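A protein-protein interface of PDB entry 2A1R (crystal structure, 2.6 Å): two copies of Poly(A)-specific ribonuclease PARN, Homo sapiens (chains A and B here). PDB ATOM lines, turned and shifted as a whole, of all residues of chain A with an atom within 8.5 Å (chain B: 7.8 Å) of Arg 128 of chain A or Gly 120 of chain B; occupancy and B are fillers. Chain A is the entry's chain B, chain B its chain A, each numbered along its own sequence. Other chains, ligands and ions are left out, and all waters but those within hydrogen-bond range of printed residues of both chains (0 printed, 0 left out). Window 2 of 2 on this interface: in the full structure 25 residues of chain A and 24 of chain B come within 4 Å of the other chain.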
ATOM      1  N   ILE A   4      32.504  12.907  26.326  1.00  0.00           N
ATOM      2  CA  ILE A   4      32.412  12.391  24.969  1.00  0.00           C
ATOM      3  C   ILE A   4      33.747  12.550  24.240  1.00  0.00           C
ATOM      4  O   ILE A   4      34.749  12.907  24.841  1.00  0.00           O
ATOM      5  CB  ILE A   4      31.282  13.092  24.226  1.00  0.00           C
ATOM      6  CG1 ILE A   4      31.588  14.576  24.069  1.00  0.00           C
ATOM      7  CG2 ILE A   4      29.953  12.887  24.981  1.00  0.00           C
ATOM      8  CD1 ILE A   4      30.507  15.363  23.376  1.00  0.00           C
ATOM      9  N   ARG A   5      33.772  12.266  22.949  1.00  0.00           N
ATOM     10  CA  ARG A   5      35.035  12.249  22.197  1.00  0.00           C
ATOM     11  C   ARG A   5      35.692  13.627  22.117  1.00  0.00           C
ATOM     12  O   ARG A   5      36.887  13.751  22.360  1.00  0.00           O
ATOM     13  CB  ARG A   5      34.814  11.677  20.787  1.00  0.00           C
ATOM     14  CG  ARG A   5      35.806  12.139  19.745  1.00  0.00           C
ATOM     15  CD  ARG A   5      36.017  11.173  18.614  1.00  0.00           C
ATOM     16  NE  ARG A   5      34.818  10.391  18.304  1.00  0.00           N
ATOM     17  CZ  ARG A   5      33.773  10.822  17.585  1.00  0.00           C
ATOM     18  NH1 ARG A   5      33.738  12.052  17.062  1.00  0.00           N
ATOM     19  NH2 ARG A   5      32.755   9.988  17.376  1.00  0.00           N
ATOM     20  N   SER A   6      34.906  14.652  21.789  1.00  0.00           N
ATOM     21  CA  SER A   6      35.423  16.026  21.650  1.00  0.00           C
ATOM     22  C   SER A   6      36.002  16.562  22.963  1.00  0.00           C
ATOM     23  O   SER A   6      36.835  17.458  22.997  1.00  0.00           O
ATOM     24  CB  SER A   6      34.310  16.971  21.151  1.00  0.00           C
ATOM     25  OG  SER A   6      33.260  17.132  22.099  1.00  0.00           O
ATOM     26  N   TYR A  91      30.921   8.118  27.381  1.00  0.00           N
ATOM     27  CA  TYR A  91      30.310   7.475  26.224  1.00  0.00           C
ATOM     28  C   TYR A  91      31.418   6.953  25.344  1.00  0.00           C
ATOM     29  O   TYR A  91      32.332   7.693  25.004  1.00  0.00           O
ATOM     30  CB  TYR A  91      29.447   8.453  25.464  1.00  0.00           C
ATOM     31  CG  TYR A  91      28.372   8.969  26.370  1.00  0.00           C
ATOM     32  CD1 TYR A  91      28.651   9.974  27.294  1.00  0.00           C
ATOM     33  CD2 TYR A  91      27.112   8.396  26.383  1.00  0.00           C
ATOM     34  CE1 TYR A  91      27.704  10.417  28.171  1.00  0.00           C
ATOM     35  CE2 TYR A  91      26.140   8.841  27.258  1.00  0.00           C
ATOM     36  CZ  TYR A  91      26.450   9.854  28.154  1.00  0.00           C
ATOM     37  OH  TYR A  91      25.531  10.314  29.043  1.00  0.00           O
ATOM     38  N   VAL A  92      31.353   5.672  25.005  1.00  0.00           N
ATOM     39  CA  VAL A  92      32.366   5.032  24.194  1.00  0.00           C
ATOM     40  C   VAL A  92      31.719   4.309  23.006  1.00  0.00           C
ATOM     41  O   VAL A  92      30.590   3.826  23.086  1.00  0.00           O
ATOM     42  CB  VAL A  92      33.188   4.030  25.035  1.00  0.00           C
ATOM     43  CG1 VAL A  92      33.739   4.696  26.241  1.00  0.00           C
ATOM     44  CG2 VAL A  92      32.353   2.830  25.487  1.00  0.00           C
ATOM     45  N   PHE A  93      32.456   4.226  21.909  1.00  0.00           N
ATOM     46  CA  PHE A  93      31.988   3.544  20.721  1.00  0.00           C
ATOM     47  C   PHE A  93      33.208   3.094  19.951  1.00  0.00           C
ATOM     48  O   PHE A  93      34.154   3.859  19.801  1.00  0.00           O
ATOM     49  CB  PHE A  93      31.140   4.494  19.862  1.00  0.00           C
ATOM     50  CG  PHE A  93      30.525   3.827  18.678  1.00  0.00           C
ATOM     51  CD1 PHE A  93      29.479   2.944  18.846  1.00  0.00           C
ATOM     52  CD2 PHE A  93      31.021   4.035  17.400  1.00  0.00           C
ATOM     53  CE1 PHE A  93      28.919   2.278  17.750  1.00  0.00           C
ATOM     54  CE2 PHE A  93      30.466   3.378  16.296  1.00  0.00           C
ATOM     55  CZ  PHE A  93      29.419   2.498  16.479  1.00  0.00           C
ATOM     56  N   LYS A  95      35.104   3.136  17.269  1.00  0.00           N
ATOM     57  CA  LYS A  95      35.347   3.745  15.967  1.00  0.00           C
ATOM     58  C   LYS A  95      36.612   3.091  15.411  1.00  0.00           C
ATOM     59  O   LYS A  95      37.664   3.164  16.051  1.00  0.00           O
ATOM     60  CB  LYS A  95      35.538   5.270  16.075  1.00  0.00           C
ATOM     61  CG  LYS A  95      35.684   5.976  14.726  1.00  0.00           C
ATOM     62  CD  LYS A  95      36.054   7.461  14.851  1.00  0.00           C
ATOM     63  CE  LYS A  95      34.955   8.313  15.511  1.00  0.00           C
ATOM     64  NZ  LYS A  95      33.717   8.466  14.667  1.00  0.00           N
ATOM     65  N   ASP A 122      20.751   9.945  25.621  1.00  0.00           N
ATOM     66  CA  ASP A 122      21.044  10.612  24.364  1.00  0.00           C
ATOM     67  C   ASP A 122      21.953   9.694  23.511  1.00  0.00           C
ATOM     68  O   ASP A 122      23.167   9.636  23.730  1.00  0.00           O
ATOM     69  CB  ASP A 122      21.702  11.968  24.635  1.00  0.00           C
ATOM     70  CG  ASP A 122      22.044  12.736  23.350  1.00  0.00           C
ATOM     71  OD1 ASP A 122      21.826  12.177  22.238  1.00  0.00           O
ATOM     72  OD2 ASP A 122      22.554  13.897  23.352  1.00  0.00           O
ATOM     73  N   PHE A 123      21.367   9.012  22.533  1.00  0.00           N
ATOM     74  CA  PHE A 123      22.114   8.090  21.684  1.00  0.00           C
ATOM     75  C   PHE A 123      23.171   8.735  20.782  1.00  0.00           C
ATOM     76  O   PHE A 123      24.106   8.076  20.363  1.00  0.00           O
ATOM     77  CB  PHE A 123      21.150   7.241  20.848  1.00  0.00           C
ATOM     78  CG  PHE A 123      20.239   6.385  21.680  1.00  0.00           C
ATOM     79  CD1 PHE A 123      18.952   6.821  22.000  1.00  0.00           C
ATOM     80  CD2 PHE A 123      20.679   5.163  22.173  1.00  0.00           C
ATOM     81  CE1 PHE A 123      18.095   6.037  22.773  1.00  0.00           C
ATOM     82  CE2 PHE A 123      19.841   4.378  22.959  1.00  0.00           C
ATOM     83  CZ  PHE A 123      18.547   4.820  23.268  1.00  0.00           C
ATOM     84  N   ASN A 124      23.031  10.020  20.485  1.00  0.00           N
ATOM     85  CA  ASN A 124      24.066  10.743  19.744  1.00  0.00           C
ATOM     86  C   ASN A 124      25.361  10.867  20.537  1.00  0.00           C
ATOM     87  O   ASN A 124      26.441  10.993  19.965  1.00  0.00           O
ATOM     88  CB  ASN A 124      23.563  12.120  19.325  1.00  0.00           C
ATOM     89  CG  ASN A 124      22.445  12.036  18.280  1.00  0.00           C
ATOM     90  OD1 ASN A 124      22.434  11.126  17.446  1.00  0.00           O
ATOM     91  ND2 ASN A 124      21.513  12.992  18.311  1.00  0.00           N
ATOM     92  N   LYS A 125      25.267  10.836  21.859  1.00  0.00           N
ATOM     93  CA  LYS A 125      26.478  10.814  22.679  1.00  0.00           C
ATOM     94  C   LYS A 125      27.311   9.549  22.431  1.00  0.00           C
ATOM     95  O   LYS A 125      28.534   9.552  22.573  1.00  0.00           O
ATOM     96  CB  LYS A 125      26.115  10.943  24.156  1.00  0.00           C
ATOM     97  CG  LYS A 125      25.559  12.311  24.494  1.00  0.00           C
ATOM     98  CD  LYS A 125      25.418  12.480  25.999  1.00  0.00           C
ATOM     99  CE  LYS A 125      24.816  13.841  26.375  1.00  0.00           C
ATOM    100  NZ  LYS A 125      24.611  13.896  27.867  1.00  0.00           N
ATOM    101  N   VAL A 126      26.647   8.473  22.032  1.00  0.00           N
ATOM    102  CA  VAL A 126      27.335   7.229  21.704  1.00  0.00           C
ATOM    103  C   VAL A 126      27.642   7.084  20.233  1.00  0.00           C
ATOM    104  O   VAL A 126      28.789   6.930  19.879  1.00  0.00           O
ATOM    105  CB  VAL A 126      26.524   6.038  22.132  1.00  0.00           C
ATOM    106  CG1 VAL A 126      27.232   4.759  21.682  1.00  0.00           C
ATOM    107  CG2 VAL A 126      26.347   6.057  23.634  1.00  0.00           C
ATOM    108  N   PHE A 127      26.619   7.109  19.381  1.00  0.00           N
ATOM    109  CA  PHE A 127      26.777   6.811  17.948  1.00  0.00           C
ATOM    110  C   PHE A 127      27.345   7.947  17.097  1.00  0.00           C
ATOM    111  O   PHE A 127      27.696   7.712  15.937  1.00  0.00           O
ATOM    112  CB  PHE A 127      25.443   6.338  17.355  1.00  0.00           C
ATOM    113  CG  PHE A 127      24.897   5.125  18.026  1.00  0.00           C
ATOM    114  CD1 PHE A 127      23.754   5.187  18.775  1.00  0.00           C
ATOM    115  CD2 PHE A 127      25.556   3.925  17.961  1.00  0.00           C
ATOM    116  CE1 PHE A 127      23.268   4.071  19.436  1.00  0.00           C
ATOM    117  CE2 PHE A 127      25.057   2.812  18.631  1.00  0.00           C
ATOM    118  CZ  PHE A 127      23.912   2.899  19.351  1.00  0.00           C
ATOM    119  N   ARG A 128      27.418   9.164  17.646  1.00  0.00           N
ATOM    120  CA  ARG A 128      28.116  10.286  16.994  1.00  0.00           C
ATOM    121  C   ARG A 128      29.322  10.755  17.788  1.00  0.00           C
ATOM    122  O   ARG A 128      30.307  11.145  17.198  1.00  0.00           O
ATOM    123  CB  ARG A 128      27.210  11.510  16.789  1.00  0.00           C
ATOM    124  CG  ARG A 128      25.874  11.259  16.131  1.00  0.00           C
ATOM    125  CD  ARG A 128      24.999  12.528  15.970  1.00  0.00           C
ATOM    126  NE  ARG A 128      25.694  13.636  15.312  1.00  0.00           N
ATOM    127  CZ  ARG A 128      25.986  13.705  14.005  1.00  0.00           C
ATOM    128  NH1 ARG A 128      25.646  12.739  13.165  1.00  0.00           N
ATOM    129  NH2 ARG A 128      26.635  14.757  13.524  1.00  0.00           N
ATOM    130  N   ASN A 129      29.241  10.769  19.114  1.00  0.00           N
ATOM    131  CA  ASN A 129      30.288  11.351  19.934  1.00  0.00           C
ATOM    132  C   ASN A 129      31.004  10.346  20.828  1.00  0.00           C
ATOM    133  O   ASN A 129      31.661  10.732  21.791  1.00  0.00           O
ATOM    134  CB  ASN A 129      29.707  12.474  20.789  1.00  0.00           C
ATOM    135  CG  ASN A 129      29.116  13.610  19.951  1.00  0.00           C
ATOM    136  OD1 ASN A 129      29.804  14.212  19.118  1.00  0.00           O
ATOM    137  ND2 ASN A 129      27.840  13.927  20.195  1.00  0.00           N
ATOM    138  N   GLY A 130      30.911   9.062  20.516  1.00  0.00           N
ATOM    139  CA  GLY A 130      31.580   8.057  21.318  1.00  0.00           C
ATOM    140  C   GLY A 130      33.091   8.229  21.376  1.00  0.00           C
ATOM    141  O   GLY A 130      33.717   8.586  20.377  1.00  0.00           O
ATOM    142  N   ILE A 131      33.674   7.996  22.549  1.00  0.00           N
ATOM    143  CA  ILE A 131      35.127   7.908  22.701  1.00  0.00           C
ATOM    144  C   ILE A 131      35.611   6.562  22.141  1.00  0.00           C
ATOM    145  O   ILE A 131      35.071   5.500  22.479  1.00  0.00           O
ATOM    146  CB  ILE A 131      35.546   8.019  24.179  1.00  0.00           C
ATOM    147  CG1 ILE A 131      34.978   9.283  24.814  1.00  0.00           C
ATOM    148  CG2 ILE A 131      37.038   8.086  24.311  1.00  0.00           C
ATOM    149  CD1 ILE A 131      34.825   9.176  26.307  1.00  0.00           C
ATOM    150  N   TYR B  91      11.435   7.560  10.052  1.00  0.00           N
ATOM    151  CA  TYR B  91      12.293   6.883  10.994  1.00  0.00           C
ATOM    152  C   TYR B  91      11.472   5.785  11.654  1.00  0.00           C
ATOM    153  O   TYR B  91      10.420   6.081  12.193  1.00  0.00           O
ATOM    154  CB  TYR B  91      12.804   7.870  12.023  1.00  0.00           C
ATOM    155  CG  TYR B  91      13.682   8.890  11.404  1.00  0.00           C
ATOM    156  CD1 TYR B  91      13.139  10.038  10.825  1.00  0.00           C
ATOM    157  CD2 TYR B  91      15.048   8.699  11.335  1.00  0.00           C
ATOM    158  CE1 TYR B  91      13.941  10.962  10.207  1.00  0.00           C
ATOM    159  CE2 TYR B  91      15.855   9.617  10.710  1.00  0.00           C
ATOM    160  CZ  TYR B  91      15.298  10.752  10.146  1.00  0.00           C
ATOM    161  OH  TYR B  91      16.110  11.698   9.536  1.00  0.00           O
ATOM    162  N   ILE B 113      27.503   2.799  11.129  1.00  0.00           N
ATOM    163  CA  ILE B 113      27.128   3.819  12.092  1.00  0.00           C
ATOM    164  C   ILE B 113      28.033   5.044  11.900  1.00  0.00           C
ATOM    165  O   ILE B 113      27.590   6.180  11.913  1.00  0.00           O
ATOM    166  CB  ILE B 113      27.229   3.261  13.535  1.00  0.00           C
ATOM    167  CG1 ILE B 113      25.877   2.717  14.023  1.00  0.00           C
ATOM    168  CG2 ILE B 113      27.597   4.355  14.510  1.00  0.00           C
ATOM    169  CD1 ILE B 113      25.216   1.694  13.140  1.00  0.00           C
ATOM    170  N   ASP B 114      29.310   4.787  11.718  1.00  0.00           N
ATOM    171  CA  ASP B 114      30.295   5.828  11.500  1.00  0.00           C
ATOM    172  C   ASP B 114      30.016   6.619  10.224  1.00  0.00           C
ATOM    173  O   ASP B 114      30.246   7.830  10.159  1.00  0.00           O
ATOM    174  CB  ASP B 114      31.670   5.189  11.383  1.00  0.00           C
ATOM    175  CG  ASP B 114      32.721   5.975  12.074  1.00  0.00           C
ATOM    176  OD1 ASP B 114      32.971   5.639  13.262  1.00  0.00           O
ATOM    177  OD2 ASP B 114      33.326   6.936  11.517  1.00  0.00           O
ATOM    178  N   PHE B 115      29.535   5.921   9.208  1.00  0.00           N
ATOM    179  CA  PHE B 115      29.241   6.551   7.945  1.00  0.00           C
ATOM    180  C   PHE B 115      27.988   7.415   8.077  1.00  0.00           C
ATOM    181  O   PHE B 115      27.952   8.550   7.618  1.00  0.00           O
ATOM    182  CB  PHE B 115      29.059   5.502   6.848  1.00  0.00           C
ATOM    183  CG  PHE B 115      28.419   6.042   5.604  1.00  0.00           C
ATOM    184  CD1 PHE B 115      29.124   6.903   4.769  1.00  0.00           C
ATOM    185  CD2 PHE B 115      27.083   5.721   5.287  1.00  0.00           C
ATOM    186  CE1 PHE B 115      28.525   7.433   3.620  1.00  0.00           C
ATOM    187  CE2 PHE B 115      26.469   6.240   4.143  1.00  0.00           C
ATOM    188  CZ  PHE B 115      27.205   7.096   3.301  1.00  0.00           C
ATOM    189  N   LEU B 116      26.958   6.867   8.704  1.00  0.00           N
ATOM    190  CA  LEU B 116      25.732   7.601   8.899  1.00  0.00           C
ATOM    191  C   LEU B 116      25.967   8.843   9.779  1.00  0.00           C
ATOM    192  O   LEU B 116      25.394   9.890   9.532  1.00  0.00           O
ATOM    193  CB  LEU B 116      24.682   6.698   9.526  1.00  0.00           C
ATOM    194  CG  LEU B 116      24.122   5.530   8.719  1.00  0.00           C
ATOM    195  CD1 LEU B 116      23.143   4.748   9.599  1.00  0.00           C
ATOM    196  CD2 LEU B 116      23.424   5.992   7.456  1.00  0.00           C
ATOM    197  N   ALA B 117      26.825   8.737  10.779  1.00  0.00           N
ATOM    198  CA  ALA B 117      27.130   9.880  11.638  1.00  0.00           C
ATOM    199  C   ALA B 117      27.807  11.010  10.875  1.00  0.00           C
ATOM    200  O   ALA B 117      27.582  12.179  11.168  1.00  0.00           O
ATOM    201  CB  ALA B 117      27.993   9.469  12.796  1.00  0.00           C
ATOM    202  N   SER B 118      28.651  10.658   9.913  1.00  0.00           N
ATOM    203  CA  SER B 118      29.414  11.660   9.171  1.00  0.00           C
ATOM    204  C   SER B 118      28.515  12.388   8.200  1.00  0.00           C
ATOM    205  O   SER B 118      28.900  13.419   7.702  1.00  0.00           O
ATOM    206  CB  SER B 118      30.568  11.016   8.386  1.00  0.00           C
ATOM    207  OG  SER B 118      30.087  10.289   7.246  1.00  0.00           O
ATOM    208  N   GLN B 119      27.354  11.809   7.892  1.00  0.00           N
ATOM    209  CA  GLN B 119      26.333  12.451   7.063  1.00  0.00           C
ATOM    210  C   GLN B 119      25.316  13.239   7.892  1.00  0.00           C
ATOM    211  O   GLN B 119      24.277  13.642   7.392  1.00  0.00           O
ATOM    212  CB  GLN B 119      25.586  11.393   6.256  1.00  0.00           C
ATOM    213  CG  GLN B 119      26.491  10.496   5.424  1.00  0.00           C
ATOM    214  CD  GLN B 119      27.332  11.282   4.447  1.00  0.00           C
ATOM    215  OE1 GLN B 119      26.796  11.920   3.534  1.00  0.00           O
ATOM    216  NE2 GLN B 119      28.644  11.273   4.647  1.00  0.00           N
ATOM    217  N   GLY B 120      25.610  13.453   9.168  1.00  0.00           N
ATOM    218  CA  GLY B 120      24.725  14.201  10.049  1.00  0.00           C
ATOM    219  C   GLY B 120      23.452  13.494  10.478  1.00  0.00           C
ATOM    220  O   GLY B 120      22.462  14.150  10.793  1.00  0.00           O
ATOM    221  N   PHE B 121      23.479  12.165  10.514  1.00  0.00           N
ATOM    222  CA  PHE B 121      22.327  11.373  10.937  1.00  0.00           C
ATOM    223  C   PHE B 121      22.047  11.629  12.428  1.00  0.00           C
ATOM    224  O   PHE B 121      22.964  11.810  13.232  1.00  0.00           O
ATOM    225  CB  PHE B 121      22.626   9.896  10.702  1.00  0.00           C
ATOM    226  CG  PHE B 121      21.419   8.987  10.715  1.00  0.00           C
ATOM    227  CD1 PHE B 121      20.655   8.831   9.583  1.00  0.00           C
ATOM    228  CD2 PHE B 121      21.111   8.224  11.837  1.00  0.00           C
ATOM    229  CE1 PHE B 121      19.592   7.974   9.562  1.00  0.00           C
ATOM    230  CE2 PHE B 121      20.043   7.348  11.837  1.00  0.00           C
ATOM    231  CZ  PHE B 121      19.277   7.217  10.705  1.00  0.00           C
ATOM    232  N   ASP B 122      20.766  11.647  12.781  1.00  0.00           N
ATOM    233  CA  ASP B 122      20.338  11.807  14.151  1.00  0.00           C
ATOM    234  C   ASP B 122      19.836  10.469  14.668  1.00  0.00           C
ATOM    235  O   ASP B 122      18.713  10.067  14.404  1.00  0.00           O
ATOM    236  CB  ASP B 122      19.235  12.866  14.256  1.00  0.00           C
ATOM    237  CG  ASP B 122      18.891  13.208  15.707  1.00  0.00           C
ATOM    238  OD1 ASP B 122      19.423  12.549  16.638  1.00  0.00           O
ATOM    239  OD2 ASP B 122      18.105  14.129  16.011  1.00  0.00           O
ATOM    240  N   PHE B 123      20.677   9.778  15.412  1.00  0.00           N
ATOM    241  CA  PHE B 123      20.302   8.482  15.935  1.00  0.00           C
ATOM    242  C   PHE B 123      19.133   8.564  16.937  1.00  0.00           C
ATOM    243  O   PHE B 123      18.439   7.587  17.122  1.00  0.00           O
ATOM    244  CB  PHE B 123      21.523   7.765  16.502  1.00  0.00           C
ATOM    245  CG  PHE B 123      22.571   7.503  15.466  1.00  0.00           C
ATOM    246  CD1 PHE B 123      23.615   8.381  15.280  1.00  0.00           C
ATOM    247  CD2 PHE B 123      22.483   6.401  14.635  1.00  0.00           C
ATOM    248  CE1 PHE B 123      24.560   8.159  14.319  1.00  0.00           C
ATOM    249  CE2 PHE B 123      23.441   6.177  13.667  1.00  0.00           C
ATOM    250  CZ  PHE B 123      24.468   7.061  13.506  1.00  0.00           C
ATOM    251  N   ASN B 124      18.902   9.721  17.559  1.00  0.00           N
ATOM    252  CA  ASN B 124      17.736   9.890  18.436  1.00  0.00           C
ATOM    253  C   ASN B 124      16.383   9.789  17.709  1.00  0.00           C
ATOM    254  O   ASN B 124      15.409   9.371  18.280  1.00  0.00           O
ATOM    255  CB  ASN B 124      17.799  11.206  19.214  1.00  0.00           C
ATOM    256  CG  ASN B 124      18.797  11.179  20.341  1.00  0.00           C
ATOM    257  OD1 ASN B 124      19.018  10.146  20.956  1.00  0.00           O
ATOM    258  ND2 ASN B 124      19.404  12.318  20.626  1.00  0.00           N
ATOM    259  N   LYS B 125      16.325  10.166  16.449  1.00  0.00           N
ATOM    260  CA  LYS B 125      15.095  10.030  15.656  1.00  0.00           C
ATOM    261  C   LYS B 125      14.707   8.578  15.445  1.00  0.00           C
ATOM    262  O   LYS B 125      13.543   8.268  15.234  1.00  0.00           O
ATOM    263  CB  LYS B 125      15.249  10.726  14.297  1.00  0.00           C
ATOM    264  CG  LYS B 125      15.536  12.197  14.457  1.00  0.00           C
ATOM    265  CD  LYS B 125      15.276  12.993  13.206  1.00  0.00           C
ATOM    266  CE  LYS B 125      15.548  14.480  13.470  1.00  0.00           C
ATOM    267  NZ  LYS B 125      15.447  15.238  12.204  1.00  0.00           N
ATOM    268  N   LEU B 376      24.438  16.116   1.977  1.00  0.00           N
ATOM    269  CA  LEU B 376      24.655  14.955   2.845  1.00  0.00           C
ATOM    270  C   LEU B 376      23.721  13.782   2.473  1.00  0.00           C
ATOM    271  O   LEU B 376      22.496  13.924   2.388  1.00  0.00           O
ATOM    272  CB  LEU B 376      24.476  15.320   4.332  1.00  0.00           C
ATOM    273  CG  LEU B 376      25.575  16.084   5.089  1.00  0.00           C
ATOM    274  CD1 LEU B 376      26.956  15.560   4.751  1.00  0.00           C
ATOM    275  CD2 LEU B 376      25.486  17.576   4.820  1.00  0.00           C
ATOM    276  N   HIS B 377      24.333  12.631   2.239  1.00  0.00           N
ATOM    277  CA  HIS B 377      23.629  11.392   1.963  1.00  0.00           C
ATOM    278  C   HIS B 377      22.524  11.138   2.981  1.00  0.00           C
ATOM    279  O   HIS B 377      22.713  11.357   4.171  1.00  0.00           O
ATOM    280  CB  HIS B 377      24.632  10.238   2.002  1.00  0.00           C
ATOM    281  CG  HIS B 377      24.010   8.887   1.842  1.00  0.00           C
ATOM    282  ND1 HIS B 377      23.466   8.447   0.654  1.00  0.00           N
ATOM    283  CD2 HIS B 377      23.839   7.879   2.734  1.00  0.00           C
ATOM    284  CE1 HIS B 377      22.988   7.224   0.825  1.00  0.00           C
ATOM    285  NE2 HIS B 377      23.206   6.855   2.073  1.00  0.00           N
ATOM    286  N   GLU B 378      21.377  10.666   2.507  1.00  0.00           N
ATOM    287  CA  GLU B 378      20.235  10.404   3.377  1.00  0.00           C
ATOM    288  C   GLU B 378      19.023   9.859   2.575  1.00  0.00           C
ATOM    289  O   GLU B 378      18.764  10.287   1.467  1.00  0.00           O
ATOM    290  CB  GLU B 378      19.920  11.671   4.179  1.00  0.00           C
ATOM    291  CG  GLU B 378      18.476  11.893   4.535  1.00  0.00           C
ATOM    292  CD  GLU B 378      17.849  12.930   3.641  1.00  0.00           C
ATOM    293  OE1 GLU B 378      18.269  14.097   3.691  1.00  0.00           O
ATOM    294  OE2 GLU B 378      16.936  12.578   2.884  1.00  0.00           O
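The backbone carbonyl oxygen of Ala 117 of chain B lies within hydrogen-bond range of the guanidinium group of Arg 128 of chain A (2.8 Å). The side-chain carboxylate (OD1) of Asp 122 of chain B is in hydrogen-bond range of the side-chain amide nitrogen (ND2) of Asn 124 of chain A (2.7 Å). NH1 of Arg 128 of chain A is in hydrogen-bond range of O of Phe 121 of chain B, at 2.8 Å. The side-chain amide oxygen of Asn 124 of chain B is in hydrogen-bond range of the backbone NH of Phe 123 of chain A. ND2 of Asn 124 of chain B lies close to ND2 of Asn 124 of chain A (3.2 Å). ND2 of Asn 124 of chain B sits at hydrogen-bond distance from OD1 of Asp 122 of chain A (2.9 Å). N of Phe 123 of chain B lies within hydrogen-bond range of OD1 of Asn 124 of chain A, at 3.0 Å. NZ of Lys 95 of chain A is in salt-bridge range of OD1 of Asp 114 of chain B (3.2 Å).
N of Phe 93 of chain A lies within hydrogen-bond range of O of Ile 131 of chain A (3.0 Å). O of Asn 124 of chain A is in hydrogen-bond range of N of Asn 129 of chain A, at 2.9 Å. The side-chain carboxylate (OD1) of Asp 122 of chain B is in hydrogen-bond range of the backbone NH (N) of Asn 124 of chain B, at 3.0 Å. The backbone NH (N) of Phe 121 of chain B sits close to the backbone carbonyl oxygen (O) of Leu 116 of chain B, 3.1 Å away. N of Asn 124 of chain A is in hydrogen-bond range of OD1 of Asp 122 of chain A (3.0 Å). The backbone carbonyl oxygen (O) of Arg 128 of chain A is in hydrogen-bond range of the guanidinium group (NH2) of Arg 5 of chain A.
Phe 93 of chain A touches Ile 113 of chain B (CZ to CG2, 3.3 Å). Phe 127 of chain A touches Ile 113 of chain B. Ala 117 of chain B touches Phe 127 of chain A. CD1 of Phe 123 of chain B touches CB of Phe 127 of chain A, at 3.4 Å. Arg 128 of chain A touches Gly 120 of chain B. CG of Arg 128 of chain A touches CD1 of Phe 123 of chain B, 3.8 Å away.
Printed residues of chain B within 4 Å of Phe 93 of chain A: Ile 113. Printed residues of chain B within 4 Å of Asn 124 of chain A: Asp 122 (2.7 Å), Phe 123 (3.0 Å) and Asn 124 (3.2 Å). Arg 128 of chain A touches four residues of chain B. Of the printed residues of chain A, Ile 113 of chain B touches Phe 93 (3.3 Å) and Phe 127 (3.6 Å). Of the printed residues of chain A, Asp 114 of chain B touches Lys 95. Of the printed residues of chain A, Ala 117 of chain B touches Phe 127 (3.6 Å) and Arg 128 (2.8 Å). Of chain A, only Arg 128 comes within 4 Å of Gly 120 of chain B. The nearest residue of chain B that does not touch Arg 128 of chain A is Leu 116 of chain B (4.6 Å). The nearest printed residue of chain A that does not touch Asp 114 of chain B is Phe 93 of chain A (4.5 Å).
Of the 17 printed residues of chain B, 8 touch a printed residue of chain A. Among the printed residues, 14 pairs touch across the chains. Among the printed residues, Asp or Glu carboxylates within 4 Å of a Lys or Arg side-chain nitrogen of the other chain: Lys 95 of chain A with Asp 114 of chain B.
Asp 122 of chain A touches Asn 124 of chain B, and with the chains exchanged Asn 124 of chain A touches Asp 122 of chain B. Phe 123 of chain A touches Asn 124 of chain B, and with the chains exchanged Asn 124 of chain A touches Phe 123 of chain B. Asn 124 of chain B touches its own counterpart, Asn 124 of chain A. Of the 14 pairs that touch across the chains among the printed residues, 5 have their exchanged pair printed and touching as well.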
